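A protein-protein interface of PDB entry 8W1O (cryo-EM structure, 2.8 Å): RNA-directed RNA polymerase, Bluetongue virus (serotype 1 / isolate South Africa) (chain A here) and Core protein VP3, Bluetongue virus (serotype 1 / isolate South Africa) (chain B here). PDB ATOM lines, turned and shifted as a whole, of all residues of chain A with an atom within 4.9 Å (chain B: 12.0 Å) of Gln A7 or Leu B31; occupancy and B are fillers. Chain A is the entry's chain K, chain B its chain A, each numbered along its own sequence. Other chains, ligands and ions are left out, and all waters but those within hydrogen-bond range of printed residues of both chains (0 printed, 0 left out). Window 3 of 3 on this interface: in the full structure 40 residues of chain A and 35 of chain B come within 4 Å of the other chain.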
ATOM      1  N   VAL A   2     -15.454  13.812  11.872  1.00  0.00           N
ATOM      2  CA  VAL A   2     -16.062  13.755  10.549  1.00  0.00           C
ATOM      3  C   VAL A   2     -16.657  15.121  10.206  1.00  0.00           C
ATOM      4  O   VAL A   2     -16.743  15.498   9.037  1.00  0.00           O
ATOM      5  CB  VAL A   2     -17.117  12.622  10.471  1.00  0.00           C
ATOM      6  CG1 VAL A   2     -18.245  12.854  11.466  1.00  0.00           C
ATOM      7  CG2 VAL A   2     -17.656  12.468   9.053  1.00  0.00           C
ATOM      8  N   ALA A   3     -17.044  15.872  11.233  1.00  0.00           N
ATOM      9  CA  ALA A   3     -17.551  17.221  11.025  1.00  0.00           C
ATOM     10  C   ALA A   3     -16.397  18.176  10.750  1.00  0.00           C
ATOM     11  O   ALA A   3     -15.361  18.124  11.421  1.00  0.00           O
ATOM     12  CB  ALA A   3     -18.346  17.682  12.244  1.00  0.00           C
ATOM     13  N   ILE A   4     -16.572  19.044   9.751  1.00  0.00           N
ATOM     14  CA  ILE A   4     -15.525  20.001   9.404  1.00  0.00           C
ATOM     15  C   ILE A   4     -15.331  21.022  10.517  1.00  0.00           C
ATOM     16  O   ILE A   4     -14.210  21.496  10.747  1.00  0.00           O
ATOM     17  CB  ILE A   4     -15.848  20.676   8.052  1.00  0.00           C
ATOM     18  CG1 ILE A   4     -14.733  21.641   7.637  1.00  0.00           C
ATOM     19  CG2 ILE A   4     -17.203  21.376   8.092  1.00  0.00           C
ATOM     20  CD1 ILE A   4     -13.360  21.008   7.577  1.00  0.00           C
ATOM     21  N   THR A   5     -16.403  21.356  11.240  1.00  0.00           N
ATOM     22  CA  THR A   5     -16.336  22.420  12.236  1.00  0.00           C
ATOM     23  C   THR A   5     -15.371  22.073  13.364  1.00  0.00           C
ATOM     24  O   THR A   5     -14.477  22.861  13.694  1.00  0.00           O
ATOM     25  CB  THR A   5     -17.731  22.705  12.792  1.00  0.00           C
ATOM     26  OG1 THR A   5     -18.392  21.468  13.086  1.00  0.00           O
ATOM     27  CG2 THR A   5     -18.557  23.484  11.782  1.00  0.00           C
ATOM     28  N   VAL A   6     -15.521  20.884  13.955  1.00  0.00           N
ATOM     29  CA  VAL A   6     -14.722  20.534  15.126  1.00  0.00           C
ATOM     30  C   VAL A   6     -13.258  20.305  14.749  1.00  0.00           C
ATOM     31  O   VAL A   6     -12.348  20.752  15.459  1.00  0.00           O
ATOM     32  CB  VAL A   6     -15.344  19.327  15.857  1.00  0.00           C
ATOM     33  CG1 VAL A   6     -15.410  18.095  14.963  1.00  0.00           C
ATOM     34  CG2 VAL A   6     -14.577  19.023  17.136  1.00  0.00           C
ATOM     35  N   GLN A   7     -13.002  19.631  13.623  1.00  0.00           N
ATOM     36  CA  GLN A   7     -11.623  19.407  13.199  1.00  0.00           C
ATOM     37  C   GLN A   7     -10.935  20.716  12.833  1.00  0.00           C
ATOM     38  O   GLN A   7      -9.773  20.938  13.199  1.00  0.00           O
ATOM     39  CB  GLN A   7     -11.579  18.426  12.028  1.00  0.00           C
ATOM     40  CG  GLN A   7     -11.540  16.961  12.446  1.00  0.00           C
ATOM     41  CD  GLN A   7     -12.835  16.480  13.063  1.00  0.00           C
ATOM     42  OE1 GLN A   7     -12.876  16.111  14.235  1.00  0.00           O
ATOM     43  NE2 GLN A   7     -13.899  16.463  12.269  1.00  0.00           N
ATOM     44  N   GLY A   8     -11.637  21.600  12.121  1.00  0.00           N
ATOM     45  CA  GLY A   8     -11.065  22.899  11.810  1.00  0.00           C
ATOM     46  C   GLY A   8     -10.794  23.725  13.052  1.00  0.00           C
ATOM     47  O   GLY A   8      -9.761  24.392  13.152  1.00  0.00           O
ATOM     48  N   ALA A   9     -11.716  23.687  14.020  1.00  0.00           N
ATOM     49  CA  ALA A   9     -11.516  24.426  15.260  1.00  0.00           C
ATOM     50  C   ALA A   9     -10.303  23.911  16.019  1.00  0.00           C
ATOM     51  O   ALA A   9      -9.491  24.702  16.511  1.00  0.00           O
ATOM     52  CB  ALA A   9     -12.771  24.341  16.127  1.00  0.00           C
ATOM     53  N   GLN A  10     -10.150  22.586  16.107  1.00  0.00           N
ATOM     54  CA  GLN A  10      -8.985  22.022  16.782  1.00  0.00           C
ATOM     55  C   GLN A  10      -7.694  22.401  16.066  1.00  0.00           C
ATOM     56  O   GLN A  10      -6.695  22.749  16.712  1.00  0.00           O
ATOM     57  CB  GLN A  10      -9.117  20.502  16.881  1.00  0.00           C
ATOM     58  CG  GLN A  10     -10.256  20.022  17.769  1.00  0.00           C
ATOM     59  CD  GLN A  10     -10.008  20.287  19.241  1.00  0.00           C
ATOM     60  OE1 GLN A  10      -8.873  20.502  19.664  1.00  0.00           O
ATOM     61  NE2 GLN A  10     -11.075  20.271  20.031  1.00  0.00           N
ATOM     62  N   LEU A  11      -7.698  22.353  14.732  1.00  0.00           N
ATOM     63  CA  LEU A  11      -6.495  22.687  13.974  1.00  0.00           C
ATOM     64  C   LEU A  11      -6.097  24.145  14.179  1.00  0.00           C
ATOM     65  O   LEU A  11      -4.923  24.451  14.427  1.00  0.00           O
ATOM     66  CB  LEU A  11      -6.715  22.390  12.490  1.00  0.00           C
ATOM     67  CG  LEU A  11      -5.511  22.630  11.577  1.00  0.00           C
ATOM     68  CD1 LEU A  11      -4.366  21.710  11.961  1.00  0.00           C
ATOM     69  CD2 LEU A  11      -5.891  22.433  10.122  1.00  0.00           C
ATOM     70  N   GLU A 160      -1.042  16.871  10.911  1.00  0.00           N
ATOM     71  CA  GLU A 160      -2.374  16.279  10.953  1.00  0.00           C
ATOM     72  C   GLU A 160      -2.627  15.321   9.793  1.00  0.00           C
ATOM     73  O   GLU A 160      -3.294  14.297   9.980  1.00  0.00           O
ATOM     74  CB  GLU A 160      -3.428  17.388  10.968  1.00  0.00           C
ATOM     75  CG  GLU A 160      -4.864  16.903  11.057  1.00  0.00           C
ATOM     76  CD  GLU A 160      -5.172  16.199  12.365  1.00  0.00           C
ATOM     77  OE1 GLU A 160      -4.496  16.485  13.374  1.00  0.00           O
ATOM     78  OE2 GLU A 160      -6.097  15.361  12.384  1.00  0.00           O
ATOM     79  N   LEU A 161      -2.111  15.624   8.600  1.00  0.00           N
ATOM     80  CA  LEU A 161      -2.324  14.769   7.438  1.00  0.00           C
ATOM     81  C   LEU A 161      -1.328  13.620   7.341  1.00  0.00           C
ATOM     82  O   LEU A 161      -1.492  12.765   6.464  1.00  0.00           O
ATOM     83  CB  LEU A 161      -2.253  15.594   6.149  1.00  0.00           C
ATOM     84  CG  LEU A 161      -3.336  16.646   5.905  1.00  0.00           C
ATOM     85  CD1 LEU A 161      -3.019  17.450   4.658  1.00  0.00           C
ATOM     86  CD2 LEU A 161      -4.699  15.992   5.784  1.00  0.00           C
ATOM     87  N   ARG A 223      -7.643  12.397  -2.860  1.00  0.00           N
ATOM     88  CA  ARG A 223      -8.265  11.559  -1.841  1.00  0.00           C
ATOM     89  C   ARG A 223      -9.781  11.531  -1.989  1.00  0.00           C
ATOM     90  O   ARG A 223     -10.417  10.506  -1.715  1.00  0.00           O
ATOM     91  CB  ARG A 223      -7.878  12.058  -0.450  1.00  0.00           C
ATOM     92  CG  ARG A 223      -8.401  11.198   0.685  1.00  0.00           C
ATOM     93  CD  ARG A 223      -7.912  11.704   2.026  1.00  0.00           C
ATOM     94  NE  ARG A 223      -8.436  10.907   3.127  1.00  0.00           N
ATOM     95  CZ  ARG A 223      -8.156  11.120   4.405  1.00  0.00           C
ATOM     96  NH1 ARG A 223      -7.380  12.123   4.784  1.00  0.00           N
ATOM     97  NH2 ARG A 223      -8.669  10.309   5.325  1.00  0.00           N
ATOM     98  N   LEU A 868     -10.751  25.277   5.487  1.00  0.00           N
ATOM     99  CA  LEU A 868      -9.682  25.381   6.477  1.00  0.00           C
ATOM    100  C   LEU A 868      -8.911  26.688   6.331  1.00  0.00           C
ATOM    101  O   LEU A 868      -8.569  27.332   7.332  1.00  0.00           O
ATOM    102  CB  LEU A 868      -8.737  24.187   6.354  1.00  0.00           C
ATOM    103  CG  LEU A 868      -9.276  22.864   6.895  1.00  0.00           C
ATOM    104  CD1 LEU A 868      -8.290  21.736   6.650  1.00  0.00           C
ATOM    105  CD2 LEU A 868      -9.589  22.996   8.372  1.00  0.00           C
ATOM    106  N   LEU B  31      -6.387  12.895   8.859  1.00  0.00           N
ATOM    107  CA  LEU B  31      -7.779  13.330   8.814  1.00  0.00           C
ATOM    108  C   LEU B  31      -8.667  12.375   8.030  1.00  0.00           C
ATOM    109  O   LEU B  31      -8.199  11.381   7.477  1.00  0.00           O
ATOM    110  CB  LEU B  31      -7.883  14.727   8.202  1.00  0.00           C
ATOM    111  CG  LEU B  31      -7.757  15.900   9.168  1.00  0.00           C
ATOM    112  CD1 LEU B  31      -7.763  17.218   8.412  1.00  0.00           C
ATOM    113  CD2 LEU B  31      -8.883  15.857  10.185  1.00  0.00           C
ATOM    114  N   SER B  32      -9.957  12.687   8.003  1.00  0.00           N
ATOM    115  CA  SER B  32     -10.928  11.965   7.200  1.00  0.00           C
ATOM    116  C   SER B  32     -11.580  12.905   6.191  1.00  0.00           C
ATOM    117  O   SER B  32     -11.516  14.130   6.315  1.00  0.00           O
ATOM    118  CB  SER B  32     -11.996  11.324   8.087  1.00  0.00           C
ATOM    119  OG  SER B  32     -11.408  10.500   9.078  1.00  0.00           O
ATOM    120  N   VAL B  33     -12.212  12.312   5.178  1.00  0.00           N
ATOM    121  CA  VAL B  33     -12.962  13.102   4.211  1.00  0.00           C
ATOM    122  C   VAL B  33     -14.207  13.667   4.882  1.00  0.00           C
ATOM    123  O   VAL B  33     -14.957  12.947   5.554  1.00  0.00           O
ATOM    124  CB  VAL B  33     -13.310  12.260   2.974  1.00  0.00           C
ATOM    125  CG1 VAL B  33     -12.063  11.999   2.148  1.00  0.00           C
ATOM    126  CG2 VAL B  33     -13.946  10.937   3.377  1.00  0.00           C
ATOM    127  N   PHE B  34     -14.419  14.973   4.726  1.00  0.00           N
ATOM    128  CA  PHE B  34     -15.552  15.629   5.364  1.00  0.00           C
ATOM    129  C   PHE B  34     -16.832  15.536   4.547  1.00  0.00           C
ATOM    130  O   PHE B  34     -17.897  15.906   5.053  1.00  0.00           O
ATOM    131  CB  PHE B  34     -15.214  17.095   5.649  1.00  0.00           C
ATOM    132  CG  PHE B  34     -14.031  17.276   6.558  1.00  0.00           C
ATOM    133  CD1 PHE B  34     -14.134  17.000   7.911  1.00  0.00           C
ATOM    134  CD2 PHE B  34     -12.816  17.717   6.062  1.00  0.00           C
ATOM    135  CE1 PHE B  34     -13.050  17.163   8.752  1.00  0.00           C
ATOM    136  CE2 PHE B  34     -11.727  17.882   6.897  1.00  0.00           C
ATOM    137  CZ  PHE B  34     -11.846  17.605   8.245  1.00  0.00           C
ATOM    138  N   ALA B  35     -16.760  15.051   3.311  1.00  0.00           N
ATOM    139  CA  ALA B  35     -17.956  14.785   2.523  1.00  0.00           C
ATOM    140  C   ALA B  35     -18.479  13.399   2.876  1.00  0.00           C
ATOM    141  O   ALA B  35     -17.732  12.417   2.820  1.00  0.00           O
ATOM    142  CB  ALA B  35     -17.652  14.890   1.031  1.00  0.00           C
ATOM    143  N   LEU B  36     -19.752  13.320   3.247  1.00  0.00           N
ATOM    144  CA  LEU B  36     -20.320  12.059   3.694  1.00  0.00           C
ATOM    145  C   LEU B  36     -20.515  11.114   2.509  1.00  0.00           C
ATOM    146  O   LEU B  36     -20.523  11.522   1.346  1.00  0.00           O
ATOM    147  CB  LEU B  36     -21.637  12.303   4.432  1.00  0.00           C
ATOM    148  CG  LEU B  36     -22.148  11.196   5.357  1.00  0.00           C
ATOM    149  CD1 LEU B  36     -21.020  10.669   6.223  1.00  0.00           C
ATOM    150  CD2 LEU B  36     -23.264  11.733   6.229  1.00  0.00           C
ATOM    151  N   GLN B  37     -20.666   9.827   2.827  1.00  0.00           N
ATOM    152  CA  GLN B  37     -20.644   8.794   1.798  1.00  0.00           C
ATOM    153  C   GLN B  37     -21.890   8.815   0.921  1.00  0.00           C
ATOM    154  O   GLN B  37     -21.860   8.277  -0.191  1.00  0.00           O
ATOM    155  CB  GLN B  37     -20.487   7.420   2.447  1.00  0.00           C
ATOM    156  CG  GLN B  37     -19.324   7.325   3.414  1.00  0.00           C
ATOM    157  CD  GLN B  37     -17.983   7.439   2.726  1.00  0.00           C
ATOM    158  OE1 GLN B  37     -17.822   7.021   1.582  1.00  0.00           O
ATOM    159  NE2 GLN B  37     -17.007   8.010   3.423  1.00  0.00           N
ATOM    160  N   MET B  40     -21.223  10.761  -2.195  1.00  0.00           N
ATOM    161  CA  MET B  40     -20.076  10.196  -2.893  1.00  0.00           C
ATOM    162  C   MET B  40     -20.441   8.904  -3.613  1.00  0.00           C
ATOM    163  O   MET B  40     -19.924   8.639  -4.703  1.00  0.00           O
ATOM    164  CB  MET B  40     -18.937   9.980  -1.898  1.00  0.00           C
ATOM    165  CG  MET B  40     -18.395  11.297  -1.352  1.00  0.00           C
ATOM    166  SD  MET B  40     -17.103  11.151  -0.106  1.00  0.00           S
ATOM    167  CE  MET B  40     -15.740  10.567  -1.095  1.00  0.00           C
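Val A2 touches Phe B34. Ala A3 touches Phe B34 (O to CE1, 3.7 Å). CD1 of Ile A4 touches CE2 of Phe B34, at 3.6 Å. CD2 of Leu B31 touches CG of Gln A7, at 3.7 Å. Gln A7 touches Phe B34 (NE2 to CE1, 3.7 Å). N of Leu B31 touches O of Glu A160 (3.6 Å). Arg A223 touches Ser B32 (NH2 to CA, 3.4 Å). Arg A223 touches Val B33.
Printed residues of chain B that touch a printed residue of chain A: Leu B31, Ser B32, Val B33 and Phe B34. Hydrophobic or aromatic side chains of chain A that line the printed part of chain B: Ile A4.
O of Leu B31 sits at hydrogen-bond distance from NH2 of Arg A223.
The backbone NH (N) of Val A2 sits close to the side-chain amide nitrogen (NE2) of Gln A7, 3.1 Å away. N of Ala A3 lies close to NE2 of Gln A7 (3.4 Å).
Of chain A, only Gln A7 (3.7 Å), Glu A160 (3.6 Å) and Arg A223 (2.4 Å) come within 4 Å of Leu B31. Of chain B, only Phe B34 comes within 4 Å of Val A2. Ile A4 touches just one residue of chain B: Phe B34. Thr A5 touches none of the printed residues of chain B. No residue of chain B comes within 4 Å of Val A6. No residue of chain B comes within 4 Å of Gly A8. No residue of chain B comes within 4 Å of Ala A9. Gln A10 touches none of the printed residues of chain B. No residue of chain B comes within 4 Å of Leu A11. Printed residues of chain B within 4 Å of Glu A160: Leu B31. No residue of chain B comes within 4 Å of Leu A161. Printed residues of chain A within 4 Å of Phe B34: Val A2 (3.2 Å), Ala A3 (3.7 Å), Ile A4 (3.6 Å) and Gln A7 (3.7 Å). Of the printed residues of chain A, Ser B32 touches Arg A223 (3.4 Å). Of the printed residues of chain A, Val B33 touches Arg A223 (3.9 Å). Of the printed residues of chain B, Arg A223 touches Leu B31, Ser B32 and Val B33. Leu A868 touches none of the printed residues of chain B. The nearest residue of chain B that does not touch Gln A7 is Ser B32 (6.4 Å). The nearest residue of chain A that does not touch Leu B31 is Leu A161 (4.2 Å).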
